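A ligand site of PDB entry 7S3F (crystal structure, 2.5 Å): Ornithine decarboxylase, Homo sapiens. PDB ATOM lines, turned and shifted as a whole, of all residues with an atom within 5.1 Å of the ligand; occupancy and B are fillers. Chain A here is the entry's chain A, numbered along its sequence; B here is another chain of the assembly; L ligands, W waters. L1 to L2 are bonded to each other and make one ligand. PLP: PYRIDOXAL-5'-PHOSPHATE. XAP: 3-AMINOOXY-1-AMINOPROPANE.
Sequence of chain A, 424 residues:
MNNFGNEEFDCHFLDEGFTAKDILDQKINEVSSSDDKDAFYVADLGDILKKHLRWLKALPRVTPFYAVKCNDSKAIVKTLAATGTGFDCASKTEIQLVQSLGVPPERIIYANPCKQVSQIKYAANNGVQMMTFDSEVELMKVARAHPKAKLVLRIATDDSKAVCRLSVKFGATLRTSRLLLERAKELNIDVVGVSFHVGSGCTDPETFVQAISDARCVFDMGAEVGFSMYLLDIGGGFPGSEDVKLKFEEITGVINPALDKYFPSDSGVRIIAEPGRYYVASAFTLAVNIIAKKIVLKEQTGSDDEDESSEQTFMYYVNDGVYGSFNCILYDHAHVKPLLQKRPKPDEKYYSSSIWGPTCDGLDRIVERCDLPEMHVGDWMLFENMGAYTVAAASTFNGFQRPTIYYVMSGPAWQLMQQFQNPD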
ATOM      1  N   ALA A  67      17.950   8.722  29.330  1.00  0.00           N
ATOM      2  CA  ALA A  67      18.603   8.388  28.057  1.00  0.00           C
ATOM      3  C   ALA A  67      19.879   9.224  27.895  1.00  0.00           C
ATOM      4  O   ALA A  67      19.852  10.348  27.398  1.00  0.00           O
ATOM      5  CB  ALA A  67      17.649   8.606  26.896  1.00  0.00           C
ATOM      6  N   LYS A  69      22.346   9.271  25.928  1.00  0.00           N
ATOM      7  CA  LYS A  69      22.713   9.754  24.599  1.00  0.00           C
ATOM      8  C   LYS A  69      22.172  11.155  24.320  1.00  0.00           C
ATOM      9  O   LYS A  69      22.712  11.877  23.480  1.00  0.00           O
ATOM     10  CB  LYS A  69      22.197   8.786  23.537  1.00  0.00           C
ATOM     11  CG  LYS A  69      20.675   8.659  23.563  1.00  0.00           C
ATOM     12  CD  LYS A  69      20.152   7.741  22.472  1.00  0.00           C
ATOM     13  CE  LYS A  69      19.009   6.859  22.932  1.00  0.00           C
ATOM     14  NZ  LYS A  69      19.452   5.827  23.905  1.00  0.00           N
ATOM     15  N   CYS A  70      21.065  11.514  24.986  1.00  0.00           N
ATOM     16  CA  CYS A  70      20.443  12.822  24.764  1.00  0.00           C
ATOM     17  C   CYS A  70      21.388  13.953  25.141  1.00  0.00           C
ATOM     18  O   CYS A  70      21.479  14.959  24.427  1.00  0.00           O
ATOM     19  CB  CYS A  70      19.163  12.910  25.579  1.00  0.00           C
ATOM     20  SG  CYS A  70      18.293  14.464  25.359  1.00  0.00           S
ATOM     21  N   ASP A  88      19.539   4.673  30.804  1.00  0.00           N
ATOM     22  CA  ASP A  88      19.485   3.966  29.529  1.00  0.00           C
ATOM     23  C   ASP A  88      20.779   4.272  28.784  1.00  0.00           C
ATOM     24  O   ASP A  88      21.013   5.415  28.356  1.00  0.00           O
ATOM     25  CB  ASP A  88      18.264   4.406  28.724  1.00  0.00           C
ATOM     26  CG  ASP A  88      18.421   4.168  27.223  1.00  0.00           C
ATOM     27  OD1 ASP A  88      19.119   3.226  26.817  1.00  0.00           O
ATOM     28  OD2 ASP A  88      17.862   4.968  26.437  1.00  0.00           O
ATOM     29  N   ALA A 111      19.862  -0.410  26.313  1.00  0.00           N
ATOM     30  CA  ALA A 111      18.671  -0.366  25.470  1.00  0.00           C
ATOM     31  C   ALA A 111      19.008  -0.023  24.022  1.00  0.00           C
ATOM     32  O   ALA A 111      18.300   0.755  23.376  1.00  0.00           O
ATOM     33  CB  ALA A 111      17.649   0.605  26.035  1.00  0.00           C
ATOM     34  N   ARG A 154      11.989  -5.417  22.155  1.00  0.00           N
ATOM     35  CA  ARG A 154      11.533  -4.130  21.664  1.00  0.00           C
ATOM     36  C   ARG A 154      10.573  -4.332  20.492  1.00  0.00           C
ATOM     37  O   ARG A 154      10.949  -4.900  19.473  1.00  0.00           O
ATOM     38  CB  ARG A 154      12.700  -3.242  21.234  1.00  0.00           C
ATOM     39  CG  ARG A 154      12.220  -1.914  20.665  1.00  0.00           C
ATOM     40  CD  ARG A 154      13.273  -0.842  20.766  1.00  0.00           C
ATOM     41  NE  ARG A 154      12.904   0.335  19.978  1.00  0.00           N
ATOM     42  CZ  ARG A 154      13.740   1.314  19.672  1.00  0.00           C
ATOM     43  NH1 ARG A 154      14.998   1.264  20.108  1.00  0.00           N
ATOM     44  NH2 ARG A 154      13.332   2.349  18.957  1.00  0.00           N
ATOM     45  N   CYS A 164      10.808  12.419  14.964  1.00  0.00           N
ATOM     46  CA  CYS A 164      11.920  11.518  14.670  1.00  0.00           C
ATOM     47  C   CYS A 164      11.394  10.094  14.718  1.00  0.00           C
ATOM     48  O   CYS A 164      11.097   9.572  15.792  1.00  0.00           O
ATOM     49  CB  CYS A 164      13.077  11.713  15.650  1.00  0.00           C
ATOM     50  SG  CYS A 164      13.656  13.438  15.823  1.00  0.00           S
ATOM     51  N   LEU A 166      11.586   6.169  14.613  1.00  0.00           N
ATOM     52  CA  LEU A 166      12.531   5.129  14.990  1.00  0.00           C
ATOM     53  C   LEU A 166      12.066   3.726  14.605  1.00  0.00           C
ATOM     54  O   LEU A 166      12.885   2.800  14.601  1.00  0.00           O
ATOM     55  CB  LEU A 166      12.791   5.186  16.498  1.00  0.00           C
ATOM     56  CG  LEU A 166      13.174   6.596  16.994  1.00  0.00           C
ATOM     57  CD1 LEU A 166      13.290   6.631  18.504  1.00  0.00           C
ATOM     58  CD2 LEU A 166      14.464   7.109  16.361  1.00  0.00           C
ATOM     59  N   HIS A 197       9.313   2.364  21.751  1.00  0.00           N
ATOM     60  CA  HIS A 197       9.569   3.801  21.664  1.00  0.00           C
ATOM     61  C   HIS A 197       8.596   4.401  20.658  1.00  0.00           C
ATOM     62  O   HIS A 197       8.665   4.089  19.468  1.00  0.00           O
ATOM     63  CB  HIS A 197      11.017   4.119  21.273  1.00  0.00           C
ATOM     64  CG  HIS A 197      11.421   5.526  21.612  1.00  0.00           C
ATOM     65  ND1 HIS A 197      10.878   6.626  20.995  1.00  0.00           N
ATOM     66  CD2 HIS A 197      12.293   6.001  22.530  1.00  0.00           C
ATOM     67  CE1 HIS A 197      11.407   7.729  21.500  1.00  0.00           C
ATOM     68  NE2 HIS A 197      12.276   7.376  22.433  1.00  0.00           N
ATOM     69  N   GLY A 199       8.513   7.281  19.436  1.00  0.00           N
ATOM     70  CA  GLY A 199       9.247   8.204  18.590  1.00  0.00           C
ATOM     71  C   GLY A 199       9.574   9.489  19.334  1.00  0.00           C
ATOM     72  O   GLY A 199       8.758  10.007  20.112  1.00  0.00           O
ATOM     73  N   SER A 200      10.778  10.007  19.103  1.00  0.00           N
ATOM     74  CA  SER A 200      11.172  11.278  19.718  1.00  0.00           C
ATOM     75  C   SER A 200      10.331  12.399  19.123  1.00  0.00           C
ATOM     76  O   SER A 200      10.181  12.496  17.898  1.00  0.00           O
ATOM     77  CB  SER A 200      12.657  11.535  19.521  1.00  0.00           C
ATOM     78  OG  SER A 200      13.170  12.362  20.557  1.00  0.00           O
ATOM     79  N   GLY A 201       9.770  13.239  19.982  1.00  0.00           N
ATOM     80  CA  GLY A 201       8.886  14.281  19.491  1.00  0.00           C
ATOM     81  C   GLY A 201       7.536  13.721  19.111  1.00  0.00           C
ATOM     82  O   GLY A 201       7.089  13.872  17.973  1.00  0.00           O
ATOM     83  N   GLY A 236      10.660   6.734  25.431  1.00  0.00           N
ATOM     84  CA  GLY A 236      10.736   8.176  25.552  1.00  0.00           C
ATOM     85  C   GLY A 236       9.721   8.891  24.672  1.00  0.00           C
ATOM     86  O   GLY A 236       8.603   8.392  24.454  1.00  0.00           O
ATOM     87  N   GLY A 237      10.096  10.067  24.170  1.00  0.00           N
ATOM     88  CA  GLY A 237       9.253  10.851  23.289  1.00  0.00           C
ATOM     89  C   GLY A 237       8.553  12.012  23.951  1.00  0.00           C
ATOM     90  O   GLY A 237       7.888  12.788  23.262  1.00  0.00           O
ATOM     91  N   PHE A 238       8.723  12.179  25.258  1.00  0.00           N
ATOM     92  CA  PHE A 238       8.072  13.250  26.000  1.00  0.00           C
ATOM     93  C   PHE A 238       8.711  14.598  25.662  1.00  0.00           C
ATOM     94  O   PHE A 238       9.921  14.677  25.459  1.00  0.00           O
ATOM     95  CB  PHE A 238       8.162  12.979  27.498  1.00  0.00           C
ATOM     96  CG  PHE A 238       7.694  11.606  27.901  1.00  0.00           C
ATOM     97  CD1 PHE A 238       6.342  11.346  28.107  1.00  0.00           C
ATOM     98  CD2 PHE A 238       8.595  10.562  28.050  1.00  0.00           C
ATOM     99  CE1 PHE A 238       5.906  10.073  28.476  1.00  0.00           C
ATOM    100  CE2 PHE A 238       8.171   9.293  28.412  1.00  0.00           C
ATOM    101  CZ  PHE A 238       6.826   9.053  28.626  1.00  0.00           C
ATOM    102  N   GLU A 274      12.263   5.624  29.412  1.00  0.00           N
ATOM    103  CA  GLU A 274      13.588   6.040  28.949  1.00  0.00           C
ATOM    104  C   GLU A 274      13.559   7.491  28.485  1.00  0.00           C
ATOM    105  O   GLU A 274      13.998   7.797  27.363  1.00  0.00           O
ATOM    106  CB  GLU A 274      14.055   5.158  27.794  1.00  0.00           C
ATOM    107  CG  GLU A 274      14.158   3.679  28.105  1.00  0.00           C
ATOM    108  CD  GLU A 274      14.326   2.809  26.860  1.00  0.00           C
ATOM    109  OE1 GLU A 274      14.112   3.313  25.723  1.00  0.00           O
ATOM    110  OE2 GLU A 274      14.653   1.608  26.992  1.00  0.00           O
ATOM    111  N   PRO A 275      13.095   8.444  29.297  1.00  0.00           N
ATOM    112  CA  PRO A 275      12.979   9.831  28.824  1.00  0.00           C
ATOM    113  C   PRO A 275      14.357  10.445  28.612  1.00  0.00           C
ATOM    114  O   PRO A 275      15.257  10.295  29.448  1.00  0.00           O
ATOM    115  CB  PRO A 275      12.239  10.539  29.963  1.00  0.00           C
ATOM    116  CG  PRO A 275      12.669   9.780  31.186  1.00  0.00           C
ATOM    117  CD  PRO A 275      12.824   8.333  30.741  1.00  0.00           C
ATOM    118  N   GLY A 276      14.546  11.062  27.447  1.00  0.00           N
ATOM    119  CA  GLY A 276      15.762  11.813  27.221  1.00  0.00           C
ATOM    120  C   GLY A 276      15.573  13.319  27.267  1.00  0.00           C
ATOM    121  O   GLY A 276      15.996  13.989  28.218  1.00  0.00           O
ATOM    122  N   ARG A 277      14.868  13.849  26.248  1.00  0.00           N
ATOM    123  CA  ARG A 277      14.775  15.301  26.104  1.00  0.00           C
ATOM    124  C   ARG A 277      13.927  15.930  27.202  1.00  0.00           C
ATOM    125  O   ARG A 277      14.107  17.121  27.512  1.00  0.00           O
ATOM    126  CB  ARG A 277      14.264  15.676  24.712  1.00  0.00           C
ATOM    127  CG  ARG A 277      12.783  15.790  24.515  1.00  0.00           C
ATOM    128  CD  ARG A 277      12.463  16.430  23.149  1.00  0.00           C
ATOM    129  NE  ARG A 277      12.815  15.537  22.038  1.00  0.00           N
ATOM    130  CZ  ARG A 277      13.635  15.853  21.043  1.00  0.00           C
ATOM    131  NH1 ARG A 277      13.928  14.949  20.120  1.00  0.00           N
ATOM    132  NH2 ARG A 277      14.174  17.065  20.970  1.00  0.00           N
ATOM    133  N   TYR A 278      13.028  15.148  27.807  1.00  0.00           N
ATOM    134  CA  TYR A 278      12.149  15.670  28.862  1.00  0.00           C
ATOM    135  C   TYR A 278      12.973  16.270  30.006  1.00  0.00           C
ATOM    136  O   TYR A 278      12.612  17.328  30.553  1.00  0.00           O
ATOM    137  CB  TYR A 278      11.229  14.577  29.402  1.00  0.00           C
ATOM    138  CG  TYR A 278      10.551  15.004  30.701  1.00  0.00           C
ATOM    139  CD1 TYR A 278       9.445  15.840  30.682  1.00  0.00           C
ATOM    140  CD2 TYR A 278      11.055  14.602  31.931  1.00  0.00           C
ATOM    141  CE1 TYR A 278       8.833  16.241  31.858  1.00  0.00           C
ATOM    142  CE2 TYR A 278      10.452  15.013  33.112  1.00  0.00           C
ATOM    143  CZ  TYR A 278       9.354  15.826  33.066  1.00  0.00           C
ATOM    144  OH  TYR A 278       8.772  16.242  34.244  1.00  0.00           O
ATOM    145  N   TYR A 331      19.829  16.854  12.288  1.00  0.00           N
ATOM    146  CA  TYR A 331      19.581  15.539  12.860  1.00  0.00           C
ATOM    147  C   TYR A 331      18.284  15.492  13.658  1.00  0.00           C
ATOM    148  O   TYR A 331      17.600  14.464  13.639  1.00  0.00           O
ATOM    149  CB  TYR A 331      20.752  15.136  13.763  1.00  0.00           C
ATOM    150  CG  TYR A 331      22.064  14.869  13.037  1.00  0.00           C
ATOM    151  CD1 TYR A 331      22.251  13.687  12.320  1.00  0.00           C
ATOM    152  CD2 TYR A 331      23.119  15.772  13.104  1.00  0.00           C
ATOM    153  CE1 TYR A 331      23.430  13.432  11.663  1.00  0.00           C
ATOM    154  CE2 TYR A 331      24.313  15.524  12.464  1.00  0.00           C
ATOM    155  CZ  TYR A 331      24.470  14.349  11.743  1.00  0.00           C
ATOM    156  OH  TYR A 331      25.657  14.104  11.091  1.00  0.00           O
ATOM    157  N   ASP A 332      17.917  16.572  14.341  1.00  0.00           N
ATOM    158  CA  ASP A 332      16.782  16.555  15.264  1.00  0.00           C
ATOM    159  C   ASP A 332      15.578  17.317  14.732  1.00  0.00           C
ATOM    160  O   ASP A 332      14.596  17.477  15.458  1.00  0.00           O
ATOM    161  CB  ASP A 332      17.197  17.111  16.629  1.00  0.00           C
ATOM    162  CG  ASP A 332      16.261  16.666  17.748  1.00  0.00           C
ATOM    163  OD1 ASP A 332      15.766  15.514  17.678  1.00  0.00           O
ATOM    164  OD2 ASP A 332      15.997  17.459  18.673  1.00  0.00           O
ATOM    165  N   TYR A 389      19.928  16.823  22.342  1.00  0.00           N
ATOM    166  CA  TYR A 389      20.460  16.508  21.014  1.00  0.00           C
ATOM    167  C   TYR A 389      21.131  17.711  20.365  1.00  0.00           C
ATOM    168  O   TYR A 389      20.947  17.981  19.178  1.00  0.00           O
ATOM    169  CB  TYR A 389      19.350  15.947  20.118  1.00  0.00           C
ATOM    170  CG  TYR A 389      18.684  14.774  20.778  1.00  0.00           C
ATOM    171  CD1 TYR A 389      19.356  13.566  20.937  1.00  0.00           C
ATOM    172  CD2 TYR A 389      17.397  14.885  21.296  1.00  0.00           C
ATOM    173  CE1 TYR A 389      18.764  12.498  21.563  1.00  0.00           C
ATOM    174  CE2 TYR A 389      16.792  13.835  21.926  1.00  0.00           C
ATOM    175  CZ  TYR A 389      17.483  12.640  22.050  1.00  0.00           C
ATOM    176  OH  TYR A 389      16.910  11.574  22.682  1.00  0.00           O
ATOM    177  N   TYR B 323      26.273   9.906  12.131  1.00  0.00           N
ATOM    178  CA  TYR B 323      26.842  10.747  13.185  1.00  0.00           C
ATOM    179  C   TYR B 323      28.352  10.663  13.227  1.00  0.00           C
ATOM    180  O   TYR B 323      28.991  11.513  13.858  1.00  0.00           O
ATOM    181  CB  TYR B 323      26.263  10.349  14.546  1.00  0.00           C
ATOM    182  CG  TYR B 323      24.814  10.767  14.728  1.00  0.00           C
ATOM    183  CD1 TYR B 323      24.484  12.025  15.219  1.00  0.00           C
ATOM    184  CD2 TYR B 323      23.772   9.887  14.412  1.00  0.00           C
ATOM    185  CE1 TYR B 323      23.169  12.420  15.371  1.00  0.00           C
ATOM    186  CE2 TYR B 323      22.446  10.256  14.574  1.00  0.00           C
ATOM    187  CZ  TYR B 323      22.147  11.532  15.058  1.00  0.00           C
ATOM    188  OH  TYR B 323      20.830  11.889  15.229  1.00  0.00           O
ATOM    189  N   CYS B 360      20.893   4.775  17.673  1.00  0.00           N
ATOM    190  CA  CYS B 360      19.459   4.572  17.857  1.00  0.00           C
ATOM    191  C   CYS B 360      18.617   5.350  16.855  1.00  0.00           C
ATOM    192  O   CYS B 360      17.443   4.997  16.651  1.00  0.00           O
ATOM    193  CB  CYS B 360      19.075   5.039  19.250  1.00  0.00           C
ATOM    194  SG  CYS B 360      19.452   6.804  19.431  1.00  0.00           S
ATOM    195  N   ASP B 361      19.155   6.415  16.280  1.00  0.00           N
ATOM    196  CA  ASP B 361      18.361   7.295  15.421  1.00  0.00           C
ATOM    197  C   ASP B 361      17.913   6.581  14.146  1.00  0.00           C
ATOM    198  O   ASP B 361      18.713   5.937  13.464  1.00  0.00           O
ATOM    199  CB  ASP B 361      19.167   8.547  15.069  1.00  0.00           C
ATOM    200  CG  ASP B 361      18.284   9.648  14.522  1.00  0.00           C
ATOM    201  OD1 ASP B 361      17.149   9.351  14.076  1.00  0.00           O
ATOM    202  OD2 ASP B 361      18.735  10.814  14.521  1.00  0.00           O
ATOM    203  N   PHE B 397      28.156  11.074  19.175  1.00  0.00           N
ATOM    204  CA  PHE B 397      26.781  10.747  19.526  1.00  0.00           C
ATOM    205  C   PHE B 397      26.646   9.252  19.839  1.00  0.00           C
ATOM    206  O   PHE B 397      27.215   8.405  19.152  1.00  0.00           O
ATOM    207  CB  PHE B 397      25.839  11.149  18.386  1.00  0.00           C
ATOM    208  CG  PHE B 397      24.376  11.031  18.732  1.00  0.00           C
ATOM    209  CD1 PHE B 397      23.834  11.763  19.786  1.00  0.00           C
ATOM    210  CD2 PHE B 397      23.538  10.205  17.986  1.00  0.00           C
ATOM    211  CE1 PHE B 397      22.472  11.671  20.100  1.00  0.00           C
ATOM    212  CE2 PHE B 397      22.179  10.106  18.287  1.00  0.00           C
ATOM    213  CZ  PHE B 397      21.646  10.839  19.344  1.00  0.00           C
HETATM  214  N1  PLP L   1      15.197   5.512  24.240  1.00  0.00           N
HETATM  215  C2  PLP L   1      15.565   5.045  22.984  1.00  0.00           C
HETATM  216  C2A PLP L   1      15.685   3.557  22.765  1.00  0.00           C
HETATM  217  C3  PLP L   1      15.816   5.954  21.931  1.00  0.00           C
HETATM  218  O3  PLP L   1      16.185   5.441  20.724  1.00  0.00           O
HETATM  219  C4  PLP L   1      15.701   7.344  22.161  1.00  0.00           C
HETATM  220  C4A PLP L   1      15.971   8.348  21.047  1.00  0.00           C
HETATM  221  C5  PLP L   1      15.318   7.757  23.450  1.00  0.00           C
HETATM  222  C6  PLP L   1      15.067   6.837  24.467  1.00  0.00           C
HETATM  223  C5A PLP L   1      15.164   9.186  23.814  1.00  0.00           C
HETATM  224  O4P PLP L   1      13.874   9.615  23.507  1.00  0.00           O
HETATM  225  P   PLP L   1      13.495  11.134  23.912  1.00  0.00           P
HETATM  226  O1P PLP L   1      12.570  11.625  22.838  1.00  0.00           O
HETATM  227  O2P PLP L   1      14.753  11.929  23.948  1.00  0.00           O
HETATM  228  O3P PLP L   1      12.891  11.058  25.277  1.00  0.00           O
HETATM  229  N1  XAP L   2      17.647  13.232  17.109  1.00  0.00           N
HETATM  230  C1  XAP L   2      16.921  12.364  18.062  1.00  0.00           C
HETATM  231  C2  XAP L   2      17.175  10.863  17.850  1.00  0.00           C
HETATM  232  C3  XAP L   2      16.529  10.122  19.016  1.00  0.00           C
HETATM  233  O1  XAP L   2      16.546   8.708  18.851  1.00  0.00           O
HETATM  234  N2  XAP L   2      16.257   7.923  19.893  1.00  0.00           N
HETATM  235  O   HOH W   1      20.037  13.887  17.218  1.00  0.00           O
HETATM  236  O   HOH W   2      11.491  12.741  26.551  1.00  0.00           O
HETATM  237  O   HOH W   3      16.076   3.942  18.750  1.00  0.00           O
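An oxygen (O1P) of PLP L1 is in hydrogen-bond range of the side-chain hydroxyl (OG) of Ser 200 (2.5 Å).
The side-chain hydroxyl of Tyr 389 is in hydrogen-bond range of an oxygen (O2P) of PLP L1.
An oxygen (O3P) of PLP L1 is in hydrogen-bond range of the backbone NH (N) of Gly 276, 2.7 Å away.
A nitrogen (N1) of PLP L1 is in hydrogen-bond range of the side-chain carboxylate (OE1) of Glu 274, at 2.9 Å.
NE2 of His 197 is in hydrogen-bond range of O4P of PLP L1, 3.0 Å away.
The backbone NH (N) of Arg 277 is in hydrogen-bond range of an oxygen (O2P) of PLP L1 (3.0 Å).
OD1 of Asp 332 lies within salt-bridge range of N1 of XAP L2.
An oxygen (O3P) of PLP L1 lies within hydrogen-bond range of the backbone NH (N) of Gly 237 (3.2 Å).
SG of Cys 360 of chain B lies within hydrogen-bond range of N2 of XAP L2, at 3.4 Å.
OD2 of Asp 361 of chain B is in salt-bridge range of N1 of XAP L2.
OG of Ser 200 is in hydrogen-bond range of NH1 of Arg 277 (2.7 Å).
The backbone carbonyl oxygen (O) of Ser 200 is in hydrogen-bond range of the backbone NH (N) of Cys 164 (3.0 Å).
NE2 of His 197 lies close to N of Gly 236, 3.5 Å away.
A ring nitrogen (ND1) of His 197 is in hydrogen-bond range of the backbone NH (N) of Gly 199.
The side-chain sulfur (SG) of Cys 70 is in hydrogen-bond range of the backbone NH (N) of Arg 277, at 3.6 Å.
The side-chain carboxylate (OD1) of Asp 332 is in hydrogen-bond range of the side-chain sulfur (SG) of Cys 164, at 3.5 Å.
The side-chain carboxylate (OD2) of Asp 88 lies within salt-bridge range of the side-chain amino group (NZ) of Lys 69 (3.1 Å).
O of Pro 275 is in hydrogen-bond range of N of Ala 67, 3.1 Å away.
The side-chain carboxylate (OD2) of Asp 88 sits close to a nitrogen (N1) of PLP L1, at 3.5 Å.
Ala 67 touches the ligand.
Lys 69 touches the ligand.
Ala 111 touches the ligand.
Arg 154 touches the ligand.
Leu 166 touches the ligand.
CA of Gly 236 touches O3P of PLP L1 (3.6 Å).
Pro 275 touches the ligand.
Tyr 331 touches the ligand.
OH of Tyr 323 of chain B touches N1 of XAP L2, 3.9 Å away.
Hydrophobic or aromatic side chains that line the ligand: Ala 67, Leu 166, His 197 and Tyr 389.
Of the 27 residues printed, 20 come within 4 Å of the ligand.
The nearest printed residue that does not touch the ligand is Cys 164 (4.1 Å).
Water W1 lies within hydrogen-bond range of a nitrogen (N1) of XAP L2 (2.5 Å) and the side-chain hydroxyl (OH) of Tyr 323 of chain B (2.9 Å).
Water W3 lies within hydrogen-bond range of an oxygen (O3) of PLP L1 (2.5 Å), the backbone carbonyl oxygen (O) of Cys 360 of chain B (2.7 Å) and the guanidinium group (NH2) of Arg 154 (3.2 Å).
Water W2 lies within hydrogen-bond range of O3P of PLP L1 (2.5 Å), O of Phe 238 (2.7 Å) and N of Tyr 278 (3.1 Å).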
